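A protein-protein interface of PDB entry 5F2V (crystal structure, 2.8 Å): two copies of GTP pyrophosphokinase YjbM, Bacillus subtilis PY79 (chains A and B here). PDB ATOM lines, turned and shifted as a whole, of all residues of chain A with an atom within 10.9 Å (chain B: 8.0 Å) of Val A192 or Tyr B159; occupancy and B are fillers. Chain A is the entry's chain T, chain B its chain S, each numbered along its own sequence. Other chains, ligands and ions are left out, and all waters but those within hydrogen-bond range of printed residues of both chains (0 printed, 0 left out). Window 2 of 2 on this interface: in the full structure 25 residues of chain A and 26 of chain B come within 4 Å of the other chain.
The side-chain hydroxyl (OH) of Tyr B157 lies within hydrogen-bond range of the side-chain carboxylate (OD2) of Asp A33 (2.5 Å).
OE1 of Glu A187 is in salt-bridge range of NE of Arg B170, 2.4 Å away.
The side-chain carboxylate (OE1) of Glu A191 sits close to the side-chain amino group (NZ) of Lys B166, 2.4 Å away.
OE1 of Gln A79 sits close to ND1 of His A35.
Gln A79 touches Ile B151.
CE of Met A185 touches CG1 of Ile B151, 3.8 Å away.
CB of Arg B170 touches CG1 of Ile A188, 3.9 Å away.
CG2 of Val B167 touches CG of Glu A191, 3.8 Å away.
Val A192 touches Leu B155 (CG2 to CD2, 3.7 Å).
Val A192 touches Lys B158 (CG1 to CE, 3.98 Å).
OH of Tyr B159 touches CA of Val A192, 3.5 Å away.
Of the printed residues of chain B, Gln A79 touches Ile B151 (3.3 Å).
Of the printed residues of chain B, Ile A188 touches Arg B170.
Of the printed residues of chain B, Val A192 touches Leu B155 (3.7 Å), Lys B158 (3.98 Å) and Tyr B159 (3.5 Å).
Gln A193 touches none of the printed residues of chain B.
Printed residues of chain A within 4 Å of Leu B155: Val A192 (3.7 Å).
Of chain A, only Val A192 comes within 4 Å of Lys B158.
No residue of chain A comes within 4 Å of Ser B160.
No residue of chain A comes within 4 Å of Asn B162.
No residue of chain A comes within 4 Å of Ile B163.
No residue of chain A comes within 4 Å of Pro B164.
Hydrophobic or aromatic side chains of chain A that line the printed part of chain B: Met A185, Ile A188 and Val A192.
Of the 18 printed residues of chain B, 8 touch a printed residue of chain A.
Printed residues of chain B that touch a printed residue of chain A: Ile B151, Leu B155, Tyr B157, Lys B158, Tyr B159, Lys B166, Val B167 and Arg B170.
Along chain B the printed residues that touch a printed residue of chain A span positions 151 to 170.
Among the printed residues, Asp or Glu carboxylates within 4 Å of a Lys or Arg side-chain nitrogen of the other chain: Glu A187 with Arg B170 and Glu A191 with Lys B166.
No position is printed for both chains.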
ATOM      1  N   ASP A  33      18.529 -33.932  -8.187  1.00  0.00           N
ATOM      2  CA  ASP A  33      19.548 -32.964  -8.593  1.00  0.00           C
ATOM      3  C   ASP A  33      18.892 -31.749  -9.262  1.00  0.00           C
ATOM      4  O   ASP A  33      19.569 -30.795  -9.664  1.00  0.00           O
ATOM      5  CB  ASP A  33      20.583 -33.614  -9.513  1.00  0.00           C
ATOM      6  CG  ASP A  33      22.003 -33.455  -8.990  1.00  0.00           C
ATOM      7  OD1 ASP A  33      22.171 -33.154  -7.787  1.00  0.00           O
ATOM      8  OD2 ASP A  33      22.952 -33.637  -9.781  1.00  0.00           O
ATOM      9  N   ASP A  34      17.562 -31.799  -9.356  1.00  0.00           N
ATOM     10  CA  ASP A  34      16.750 -30.717  -9.886  1.00  0.00           C
ATOM     11  C   ASP A  34      16.778 -29.550  -8.899  1.00  0.00           C
ATOM     12  O   ASP A  34      17.073 -29.745  -7.713  1.00  0.00           O
ATOM     13  CB  ASP A  34      15.317 -31.207 -10.137  1.00  0.00           C
ATOM     14  CG  ASP A  34      14.514 -30.249 -10.983  1.00  0.00           C
ATOM     15  OD1 ASP A  34      15.129 -29.366 -11.605  1.00  0.00           O
ATOM     16  OD2 ASP A  34      13.273 -30.380 -11.034  1.00  0.00           O
ATOM     17  N   HIS A  35      16.493 -28.345  -9.391  1.00  0.00           N
ATOM     18  CA  HIS A  35      16.499 -27.148  -8.558  1.00  0.00           C
ATOM     19  C   HIS A  35      15.414 -27.247  -7.484  1.00  0.00           C
ATOM     20  O   HIS A  35      14.237 -27.474  -7.782  1.00  0.00           O
ATOM     21  CB  HIS A  35      16.315 -25.890  -9.422  1.00  0.00           C
ATOM     22  CG  HIS A  35      15.745 -24.711  -8.688  1.00  0.00           C
ATOM     23  ND1 HIS A  35      16.492 -23.925  -7.835  1.00  0.00           N
ATOM     24  CD2 HIS A  35      14.498 -24.173  -8.697  1.00  0.00           C
ATOM     25  CE1 HIS A  35      15.729 -22.962  -7.344  1.00  0.00           C
ATOM     26  NE2 HIS A  35      14.514 -23.094  -7.845  1.00  0.00           N
ATOM     27  N   GLN A  79      15.142 -18.862  -4.227  1.00  0.00           N
ATOM     28  CA  GLN A  79      16.029 -18.097  -5.096  1.00  0.00           C
ATOM     29  C   GLN A  79      15.215 -17.226  -6.035  1.00  0.00           C
ATOM     30  O   GLN A  79      15.485 -16.035  -6.174  1.00  0.00           O
ATOM     31  CB  GLN A  79      16.945 -19.026  -5.892  1.00  0.00           C
ATOM     32  CG  GLN A  79      18.129 -19.558  -5.095  1.00  0.00           C
ATOM     33  CD  GLN A  79      18.802 -20.749  -5.759  1.00  0.00           C
ATOM     34  OE1 GLN A  79      18.257 -21.347  -6.686  1.00  0.00           O
ATOM     35  NE2 GLN A  79      19.986 -21.110  -5.274  1.00  0.00           N
ATOM     36  N   PHE A  80      14.190 -17.822  -6.636  1.00  0.00           N
ATOM     37  CA  PHE A  80      13.474 -17.213  -7.748  1.00  0.00           C
ATOM     38  C   PHE A  80      11.999 -16.894  -7.478  1.00  0.00           C
ATOM     39  O   PHE A  80      11.263 -17.705  -6.932  1.00  0.00           O
ATOM     40  CB  PHE A  80      13.585 -18.127  -8.968  1.00  0.00           C
ATOM     41  CG  PHE A  80      15.000 -18.484  -9.327  1.00  0.00           C
ATOM     42  CD1 PHE A  80      15.848 -17.542  -9.877  1.00  0.00           C
ATOM     43  CD2 PHE A  80      15.480 -19.761  -9.123  1.00  0.00           C
ATOM     44  CE1 PHE A  80      17.153 -17.866 -10.206  1.00  0.00           C
ATOM     45  CE2 PHE A  80      16.772 -20.090  -9.449  1.00  0.00           C
ATOM     46  CZ  PHE A  80      17.616 -19.139  -9.994  1.00  0.00           C
ATOM     47  N   GLU A 184      17.230  -9.641 -12.376  1.00  0.00           N
ATOM     48  CA  GLU A 184      18.290 -10.329 -13.101  1.00  0.00           C
ATOM     49  C   GLU A 184      18.356 -11.824 -12.808  1.00  0.00           C
ATOM     50  O   GLU A 184      18.785 -12.596 -13.659  1.00  0.00           O
ATOM     51  CB  GLU A 184      19.639  -9.687 -12.798  1.00  0.00           C
ATOM     52  CG  GLU A 184      19.708  -8.191 -13.121  1.00  0.00           C
ATOM     53  CD  GLU A 184      19.294  -7.843 -14.552  1.00  0.00           C
ATOM     54  OE1 GLU A 184      19.686  -8.567 -15.499  1.00  0.00           O
ATOM     55  OE2 GLU A 184      18.567  -6.832 -14.715  1.00  0.00           O
ATOM     56  N   MET A 185      17.926 -12.252 -11.625  1.00  0.00           N
ATOM     57  CA  MET A 185      17.890 -13.686 -11.345  1.00  0.00           C
ATOM     58  C   MET A 185      16.757 -14.358 -12.105  1.00  0.00           C
ATOM     59  O   MET A 185      16.952 -15.420 -12.677  1.00  0.00           O
ATOM     60  CB  MET A 185      17.756 -13.948  -9.852  1.00  0.00           C
ATOM     61  CG  MET A 185      18.881 -13.372  -9.023  1.00  0.00           C
ATOM     62  SD  MET A 185      20.103 -14.600  -8.568  1.00  0.00           S
ATOM     63  CE  MET A 185      20.613 -15.164 -10.177  1.00  0.00           C
ATOM     64  N   SER A 186      15.579 -13.741 -12.133  1.00  0.00           N
ATOM     65  CA  SER A 186      14.463 -14.309 -12.891  1.00  0.00           C
ATOM     66  C   SER A 186      14.837 -14.484 -14.355  1.00  0.00           C
ATOM     67  O   SER A 186      14.363 -15.415 -15.017  1.00  0.00           O
ATOM     68  CB  SER A 186      13.219 -13.438 -12.783  1.00  0.00           C
ATOM     69  OG  SER A 186      12.776 -13.349 -11.447  1.00  0.00           O
ATOM     70  N   GLU A 187      15.702 -13.588 -14.847  1.00  0.00           N
ATOM     71  CA  GLU A 187      16.184 -13.643 -16.226  1.00  0.00           C
ATOM     72  C   GLU A 187      17.210 -14.752 -16.438  1.00  0.00           C
ATOM     73  O   GLU A 187      17.270 -15.350 -17.517  1.00  0.00           O
ATOM     74  CB  GLU A 187      16.773 -12.299 -16.640  1.00  0.00           C
ATOM     75  CG  GLU A 187      15.735 -11.296 -17.130  1.00  0.00           C
ATOM     76  CD  GLU A 187      16.321 -10.313 -18.108  1.00  0.00           C
ATOM     77  OE1 GLU A 187      16.994 -10.767 -19.056  1.00  0.00           O
ATOM     78  OE2 GLU A 187      16.123  -9.090 -17.927  1.00  0.00           O
ATOM     79  N   ILE A 188      18.014 -15.018 -15.411  1.00  0.00           N
ATOM     80  CA  ILE A 188      18.848 -16.222 -15.378  1.00  0.00           C
ATOM     81  C   ILE A 188      17.987 -17.476 -15.534  1.00  0.00           C
ATOM     82  O   ILE A 188      18.030 -18.124 -16.573  1.00  0.00           O
ATOM     83  CB  ILE A 188      19.666 -16.322 -14.066  1.00  0.00           C
ATOM     84  CG1 ILE A 188      20.772 -15.270 -14.055  1.00  0.00           C
ATOM     85  CG2 ILE A 188      20.262 -17.724 -13.889  1.00  0.00           C
ATOM     86  CD1 ILE A 188      21.742 -15.436 -12.920  1.00  0.00           C
ATOM     87  N   ARG A 189      17.201 -17.796 -14.503  1.00  0.00           N
ATOM     88  CA  ARG A 189      16.327 -18.980 -14.502  1.00  0.00           C
ATOM     89  C   ARG A 189      15.455 -19.004 -15.751  1.00  0.00           C
ATOM     90  O   ARG A 189      15.012 -20.075 -16.187  1.00  0.00           O
ATOM     91  CB  ARG A 189      15.446 -19.019 -13.245  1.00  0.00           C
ATOM     92  CG  ARG A 189      14.428 -20.165 -13.194  1.00  0.00           C
ATOM     93  CD  ARG A 189      15.058 -21.510 -12.771  1.00  0.00           C
ATOM     94  NE  ARG A 189      14.069 -22.595 -12.677  1.00  0.00           N
ATOM     95  CZ  ARG A 189      14.337 -23.853 -12.309  1.00  0.00           C
ATOM     96  NH1 ARG A 189      15.575 -24.221 -11.989  1.00  0.00           N
ATOM     97  NH2 ARG A 189      13.361 -24.753 -12.262  1.00  0.00           N
ATOM     98  N   GLY A 190      15.219 -17.821 -16.323  1.00  0.00           N
ATOM     99  CA  GLY A 190      14.478 -17.709 -17.561  1.00  0.00           C
ATOM    100  C   GLY A 190      15.300 -18.226 -18.722  1.00  0.00           C
ATOM    101  O   GLY A 190      14.854 -19.082 -19.484  1.00  0.00           O
ATOM    102  N   GLU A 191      16.520 -17.714 -18.844  1.00  0.00           N
ATOM    103  CA  GLU A 191      17.403 -18.062 -19.955  1.00  0.00           C
ATOM    104  C   GLU A 191      17.819 -19.542 -19.945  1.00  0.00           C
ATOM    105  O   GLU A 191      18.033 -20.147 -21.000  1.00  0.00           O
ATOM    106  CB  GLU A 191      18.641 -17.166 -19.932  1.00  0.00           C
ATOM    107  CG  GLU A 191      19.435 -17.247 -21.203  1.00  0.00           C
ATOM    108  CD  GLU A 191      18.530 -17.384 -22.408  1.00  0.00           C
ATOM    109  OE1 GLU A 191      17.690 -16.482 -22.623  1.00  0.00           O
ATOM    110  OE2 GLU A 191      18.641 -18.405 -23.124  1.00  0.00           O
ATOM    111  N   VAL A 192      17.922 -20.115 -18.750  1.00  0.00           N
ATOM    112  CA  VAL A 192      18.260 -21.523 -18.593  1.00  0.00           C
ATOM    113  C   VAL A 192      17.236 -22.425 -19.249  1.00  0.00           C
ATOM    114  O   VAL A 192      17.576 -23.260 -20.091  1.00  0.00           O
ATOM    115  CB  VAL A 192      18.373 -21.921 -17.105  1.00  0.00           C
ATOM    116  CG1 VAL A 192      18.186 -23.423 -16.940  1.00  0.00           C
ATOM    117  CG2 VAL A 192      19.711 -21.472 -16.534  1.00  0.00           C
ATOM    118  N   GLN A 193      15.977 -22.243 -18.865  1.00  0.00           N
ATOM    119  CA  GLN A 193      14.906 -23.147 -19.276  1.00  0.00           C
ATOM    120  C   GLN A 193      14.646 -23.058 -20.778  1.00  0.00           C
ATOM    121  O   GLN A 193      13.868 -23.831 -21.337  1.00  0.00           O
ATOM    122  CB  GLN A 193      13.640 -22.860 -18.464  1.00  0.00           C
ATOM    123  CG  GLN A 193      13.846 -23.144 -16.976  1.00  0.00           C
ATOM    124  CD  GLN A 193      12.589 -22.970 -16.146  1.00  0.00           C
ATOM    125  OE1 GLN A 193      12.170 -21.846 -15.861  1.00  0.00           O
ATOM    126  NE2 GLN A 193      11.983 -24.087 -15.744  1.00  0.00           N
ATOM    127  N   GLU A 194      15.325 -22.113 -21.422  1.00  0.00           N
ATOM    128  CA  GLU A 194      15.500 -22.140 -22.866  1.00  0.00           C
ATOM    129  C   GLU A 194      16.559 -23.209 -23.196  1.00  0.00           C
ATOM    130  O   GLU A 194      17.663 -22.898 -23.655  1.00  0.00           O
ATOM    131  CB  GLU A 194      15.911 -20.757 -23.382  1.00  0.00           C
ATOM    132  CG  GLU A 194      15.557 -20.501 -24.839  1.00  0.00           C
ATOM    133  CD  GLU A 194      14.790 -19.198 -25.051  1.00  0.00           C
ATOM    134  OE1 GLU A 194      14.619 -18.425 -24.083  1.00  0.00           O
ATOM    135  OE2 GLU A 194      14.354 -18.948 -26.195  1.00  0.00           O
ATOM    136  N   ALA A 195      16.211 -24.471 -22.935  1.00  0.00           N
ATOM    137  CA  ALA A 195      17.146 -25.588 -23.048  1.00  0.00           C
ATOM    138  C   ALA A 195      16.908 -26.400 -24.322  1.00  0.00           C
ATOM    139  O   ALA A 195      17.794 -27.117 -24.796  1.00  0.00           O
ATOM    140  CB  ALA A 195      17.039 -26.487 -21.815  1.00  0.00           C
ATOM    141  N   ILE B 151      24.328 -19.500  -7.402  1.00  0.00           N
ATOM    142  CA  ILE B 151      23.744 -19.733  -8.722  1.00  0.00           C
ATOM    143  C   ILE B 151      24.853 -20.017  -9.708  1.00  0.00           C
ATOM    144  O   ILE B 151      24.753 -20.938 -10.521  1.00  0.00           O
ATOM    145  CB  ILE B 151      22.937 -18.551  -9.235  1.00  0.00           C
ATOM    146  CG1 ILE B 151      21.953 -18.090  -8.176  1.00  0.00           C
ATOM    147  CG2 ILE B 151      22.180 -18.957 -10.462  1.00  0.00           C
ATOM    148  CD1 ILE B 151      21.012 -19.181  -7.735  1.00  0.00           C
ATOM    149  N   GLU B 152      25.918 -19.228  -9.621  1.00  0.00           N
ATOM    150  CA  GLU B 152      27.089 -19.467 -10.442  1.00  0.00           C
ATOM    151  C   GLU B 152      27.605 -20.893 -10.295  1.00  0.00           C
ATOM    152  O   GLU B 152      27.861 -21.555 -11.289  1.00  0.00           O
ATOM    153  CB  GLU B 152      28.190 -18.476 -10.097  1.00  0.00           C
ATOM    154  CG  GLU B 152      29.188 -18.261 -11.220  1.00  0.00           C
ATOM    155  CD  GLU B 152      30.460 -19.061 -11.034  1.00  0.00           C
ATOM    156  OE1 GLU B 152      30.604 -19.720  -9.976  1.00  0.00           O
ATOM    157  OE2 GLU B 152      31.315 -19.024 -11.949  1.00  0.00           O
ATOM    158  N   HIS B 153      27.750 -21.380  -9.067  1.00  0.00           N
ATOM    159  CA  HIS B 153      28.215 -22.749  -8.882  1.00  0.00           C
ATOM    160  C   HIS B 153      27.263 -23.773  -9.524  1.00  0.00           C
ATOM    161  O   HIS B 153      27.711 -24.679 -10.233  1.00  0.00           O
ATOM    162  CB  HIS B 153      28.405 -23.080  -7.398  1.00  0.00           C
ATOM    163  CG  HIS B 153      28.800 -24.507  -7.149  1.00  0.00           C
ATOM    164  ND1 HIS B 153      27.883 -25.539  -7.095  1.00  0.00           N
ATOM    165  CD2 HIS B 153      30.015 -25.075  -6.952  1.00  0.00           C
ATOM    166  CE1 HIS B 153      28.513 -26.678  -6.870  1.00  0.00           C
ATOM    167  NE2 HIS B 153      29.807 -26.425  -6.780  1.00  0.00           N
ATOM    168  N   SER B 154      25.962 -23.639  -9.274  1.00  0.00           N
ATOM    169  CA  SER B 154      24.976 -24.564  -9.844  1.00  0.00           C
ATOM    170  C   SER B 154      25.113 -24.694 -11.358  1.00  0.00           C
ATOM    171  O   SER B 154      25.383 -25.780 -11.872  1.00  0.00           O
ATOM    172  CB  SER B 154      23.568 -24.106  -9.502  1.00  0.00           C
ATOM    173  OG  SER B 154      23.540 -23.618  -8.177  1.00  0.00           O
ATOM    174  N   LEU B 155      24.918 -23.572 -12.054  1.00  0.00           N
ATOM    175  CA  LEU B 155      25.092 -23.469 -13.503  1.00  0.00           C
ATOM    176  C   LEU B 155      26.434 -24.039 -13.964  1.00  0.00           C
ATOM    177  O   LEU B 155      26.502 -24.822 -14.906  1.00  0.00           O
ATOM    178  CB  LEU B 155      24.972 -22.002 -13.944  1.00  0.00           C
ATOM    179  CG  LEU B 155      23.747 -21.211 -13.474  1.00  0.00           C
ATOM    180  CD1 LEU B 155      23.915 -19.733 -13.786  1.00  0.00           C
ATOM    181  CD2 LEU B 155      22.472 -21.737 -14.090  1.00  0.00           C
ATOM    182  N   ASN B 156      27.504 -23.648 -13.290  1.00  0.00           N
ATOM    183  CA  ASN B 156      28.833 -24.148 -13.618  1.00  0.00           C
ATOM    184  C   ASN B 156      28.937 -25.676 -13.524  1.00  0.00           C
ATOM    185  O   ASN B 156      29.945 -26.266 -13.902  1.00  0.00           O
ATOM    186  CB  ASN B 156      29.865 -23.506 -12.702  1.00  0.00           C
ATOM    187  CG  ASN B 156      31.077 -23.032 -13.446  1.00  0.00           C
ATOM    188  OD1 ASN B 156      32.061 -23.753 -13.576  1.00  0.00           O
ATOM    189  ND2 ASN B 156      31.013 -21.812 -13.948  1.00  0.00           N
ATOM    190  N   TYR B 157      27.890 -26.299 -12.999  1.00  0.00           N
ATOM    191  CA  TYR B 157      27.779 -27.745 -12.945  1.00  0.00           C
ATOM    192  C   TYR B 157      26.801 -28.243 -14.010  1.00  0.00           C
ATOM    193  O   TYR B 157      27.074 -29.228 -14.700  1.00  0.00           O
ATOM    194  CB  TYR B 157      27.331 -28.195 -11.547  1.00  0.00           C
ATOM    195  CG  TYR B 157      26.613 -29.527 -11.540  1.00  0.00           C
ATOM    196  CD1 TYR B 157      25.250 -29.601 -11.817  1.00  0.00           C
ATOM    197  CD2 TYR B 157      27.292 -30.705 -11.262  1.00  0.00           C
ATOM    198  CE1 TYR B 157      24.586 -30.804 -11.826  1.00  0.00           C
ATOM    199  CE2 TYR B 157      26.636 -31.914 -11.268  1.00  0.00           C
ATOM    200  CZ  TYR B 157      25.279 -31.957 -11.550  1.00  0.00           C
ATOM    201  OH  TYR B 157      24.602 -33.156 -11.560  1.00  0.00           O
ATOM    202  N   LYS B 158      25.654 -27.569 -14.110  1.00  0.00           N
ATOM    203  CA  LYS B 158      24.632 -27.863 -15.117  1.00  0.00           C
ATOM    204  C   LYS B 158      25.241 -27.877 -16.521  1.00  0.00           C
ATOM    205  O   LYS B 158      25.117 -28.866 -17.249  1.00  0.00           O
ATOM    206  CB  LYS B 158      23.488 -26.838 -15.042  1.00  0.00           C
ATOM    207  CG  LYS B 158      22.243 -27.200 -15.861  1.00  0.00           C
ATOM    208  CD  LYS B 158      21.136 -26.142 -15.730  1.00  0.00           C
ATOM    209  CE  LYS B 158      19.747 -26.747 -15.407  1.00  0.00           C
ATOM    210  NZ  LYS B 158      19.610 -27.299 -14.014  1.00  0.00           N
ATOM    211  N   TYR B 159      25.911 -26.782 -16.883  1.00  0.00           N
ATOM    212  CA  TYR B 159      26.575 -26.659 -18.183  1.00  0.00           C
ATOM    213  C   TYR B 159      28.028 -27.114 -18.085  1.00  0.00           C
ATOM    214  O   TYR B 159      28.889 -26.705 -18.870  1.00  0.00           O
ATOM    215  CB  TYR B 159      26.475 -25.223 -18.707  1.00  0.00           C
ATOM    216  CG  TYR B 159      25.042 -24.758 -18.855  1.00  0.00           C
ATOM    217  CD1 TYR B 159      24.212 -25.296 -19.832  1.00  0.00           C
ATOM    218  CD2 TYR B 159      24.515 -23.790 -18.010  1.00  0.00           C
ATOM    219  CE1 TYR B 159      22.893 -24.880 -19.965  1.00  0.00           C
ATOM    220  CE2 TYR B 159      23.196 -23.368 -18.133  1.00  0.00           C
ATOM    221  CZ  TYR B 159      22.391 -23.915 -19.110  1.00  0.00           C
ATOM    222  OH  TYR B 159      21.084 -23.493 -19.229  1.00  0.00           O
ATOM    223  N   SER B 160      28.277 -27.961 -17.090  1.00  0.00           N
ATOM    224  CA  SER B 160      29.491 -28.774 -16.997  1.00  0.00           C
ATOM    225  C   SER B 160      30.793 -27.996 -17.190  1.00  0.00           C
ATOM    226  O   SER B 160      31.786 -28.551 -17.656  1.00  0.00           O
ATOM    227  CB  SER B 160      29.423 -29.924 -18.013  1.00  0.00           C
ATOM    228  OG  SER B 160      28.253 -30.705 -17.816  1.00  0.00           O
ATOM    229  N   GLY B 161      30.787 -26.721 -16.824  1.00  0.00           N
ATOM    230  CA  GLY B 161      31.995 -25.923 -16.872  1.00  0.00           C
ATOM    231  C   GLY B 161      31.976 -24.975 -18.047  1.00  0.00           C
ATOM    232  O   GLY B 161      32.742 -24.000 -18.104  1.00  0.00           O
ATOM    233  N   ASN B 162      31.092 -25.271 -18.995  1.00  0.00           N
ATOM    234  CA  ASN B 162      30.909 -24.414 -20.162  1.00  0.00           C
ATOM    235  C   ASN B 162      29.508 -23.817 -20.217  1.00  0.00           C
ATOM    236  O   ASN B 162      28.582 -24.409 -20.783  1.00  0.00           O
ATOM    237  CB  ASN B 162      31.189 -25.189 -21.448  1.00  0.00           C
ATOM    238  CG  ASN B 162      31.942 -24.360 -22.459  1.00  0.00           C
ATOM    239  OD1 ASN B 162      32.623 -23.397 -22.100  1.00  0.00           O
ATOM    240  ND2 ASN B 162      31.823 -24.723 -23.735  1.00  0.00           N
ATOM    241  N   ILE B 163      29.361 -22.643 -19.619  1.00  0.00           N
ATOM    242  CA  ILE B 163      28.081 -21.955 -19.627  1.00  0.00           C
ATOM    243  C   ILE B 163      27.864 -21.236 -20.957  1.00  0.00           C
ATOM    244  O   ILE B 163      28.758 -20.534 -21.448  1.00  0.00           O
ATOM    245  CB  ILE B 163      27.978 -20.942 -18.468  1.00  0.00           C
ATOM    246  CG1 ILE B 163      28.139 -21.664 -17.129  1.00  0.00           C
ATOM    247  CG2 ILE B 163      26.648 -20.186 -18.529  1.00  0.00           C
ATOM    248  CD1 ILE B 163      28.079 -20.759 -15.925  1.00  0.00           C
ATOM    249  N   PRO B 164      26.672 -21.424 -21.547  1.00  0.00           N
ATOM    250  CA  PRO B 164      26.217 -20.706 -22.741  1.00  0.00           C
ATOM    251  C   PRO B 164      26.439 -19.202 -22.616  1.00  0.00           C
ATOM    252  O   PRO B 164      26.544 -18.664 -21.512  1.00  0.00           O
ATOM    253  CB  PRO B 164      24.719 -21.038 -22.811  1.00  0.00           C
ATOM    254  CG  PRO B 164      24.388 -21.700 -21.497  1.00  0.00           C
ATOM    255  CD  PRO B 164      25.648 -22.353 -21.044  1.00  0.00           C
ATOM    256  N   LYS B 166      24.481 -16.563 -23.623  1.00  0.00           N
ATOM    257  CA  LYS B 166      23.322 -15.804 -23.179  1.00  0.00           C
ATOM    258  C   LYS B 166      23.201 -15.857 -21.650  1.00  0.00           C
ATOM    259  O   LYS B 166      22.959 -14.836 -21.002  1.00  0.00           O
ATOM    260  CB  LYS B 166      22.049 -16.327 -23.851  1.00  0.00           C
ATOM    261  CG  LYS B 166      20.848 -15.401 -23.695  1.00  0.00           C
ATOM    262  CD  LYS B 166      20.000 -15.342 -24.966  1.00  0.00           C
ATOM    263  CE  LYS B 166      18.913 -14.279 -24.849  1.00  0.00           C
ATOM    264  NZ  LYS B 166      18.269 -14.342 -23.496  1.00  0.00           N
ATOM    265  N   VAL B 167      23.397 -17.044 -21.080  1.00  0.00           N
ATOM    266  CA  VAL B 167      23.333 -17.214 -19.633  1.00  0.00           C
ATOM    267  C   VAL B 167      24.482 -16.463 -18.957  1.00  0.00           C
ATOM    268  O   VAL B 167      24.252 -15.692 -18.025  1.00  0.00           O
ATOM    269  CB  VAL B 167      23.358 -18.705 -19.236  1.00  0.00           C
ATOM    270  CG1 VAL B 167      23.329 -18.868 -17.722  1.00  0.00           C
ATOM    271  CG2 VAL B 167      22.181 -19.421 -19.853  1.00  0.00           C
ATOM    272  N   LYS B 168      25.710 -16.663 -19.438  1.00  0.00           N
ATOM    273  CA  LYS B 168      26.879 -15.976 -18.869  1.00  0.00           C
ATOM    274  C   LYS B 168      26.679 -14.470 -18.631  1.00  0.00           C
ATOM    275  O   LYS B 168      27.092 -13.954 -17.597  1.00  0.00           O
ATOM    276  CB  LYS B 168      28.104 -16.180 -19.760  1.00  0.00           C
ATOM    277  CG  LYS B 168      28.717 -17.564 -19.664  1.00  0.00           C
ATOM    278  CD  LYS B 168      30.141 -17.574 -20.191  1.00  0.00           C
ATOM    279  CE  LYS B 168      30.884 -18.789 -19.678  1.00  0.00           C
ATOM    280  NZ  LYS B 168      30.813 -18.866 -18.187  1.00  0.00           N
ATOM    281  N   ARG B 170      23.659 -12.749 -18.266  1.00  0.00           N
ATOM    282  CA  ARG B 170      22.688 -12.543 -17.211  1.00  0.00           C
ATOM    283  C   ARG B 170      23.392 -12.789 -15.877  1.00  0.00           C
ATOM    284  O   ARG B 170      23.083 -12.148 -14.869  1.00  0.00           O
ATOM    285  CB  ARG B 170      21.473 -13.462 -17.387  1.00  0.00           C
ATOM    286  CG  ARG B 170      20.756 -13.339 -18.736  1.00  0.00           C
ATOM    287  CD  ARG B 170      20.309 -11.898 -19.045  1.00  0.00           C
ATOM    288  NE  ARG B 170      19.036 -11.869 -19.767  1.00  0.00           N
ATOM    289  CZ  ARG B 170      18.900 -12.062 -21.076  1.00  0.00           C
ATOM    290  NH1 ARG B 170      19.963 -12.296 -21.830  1.00  0.00           N
ATOM    291  NH2 ARG B 170      17.696 -12.020 -21.631  1.00  0.00           N
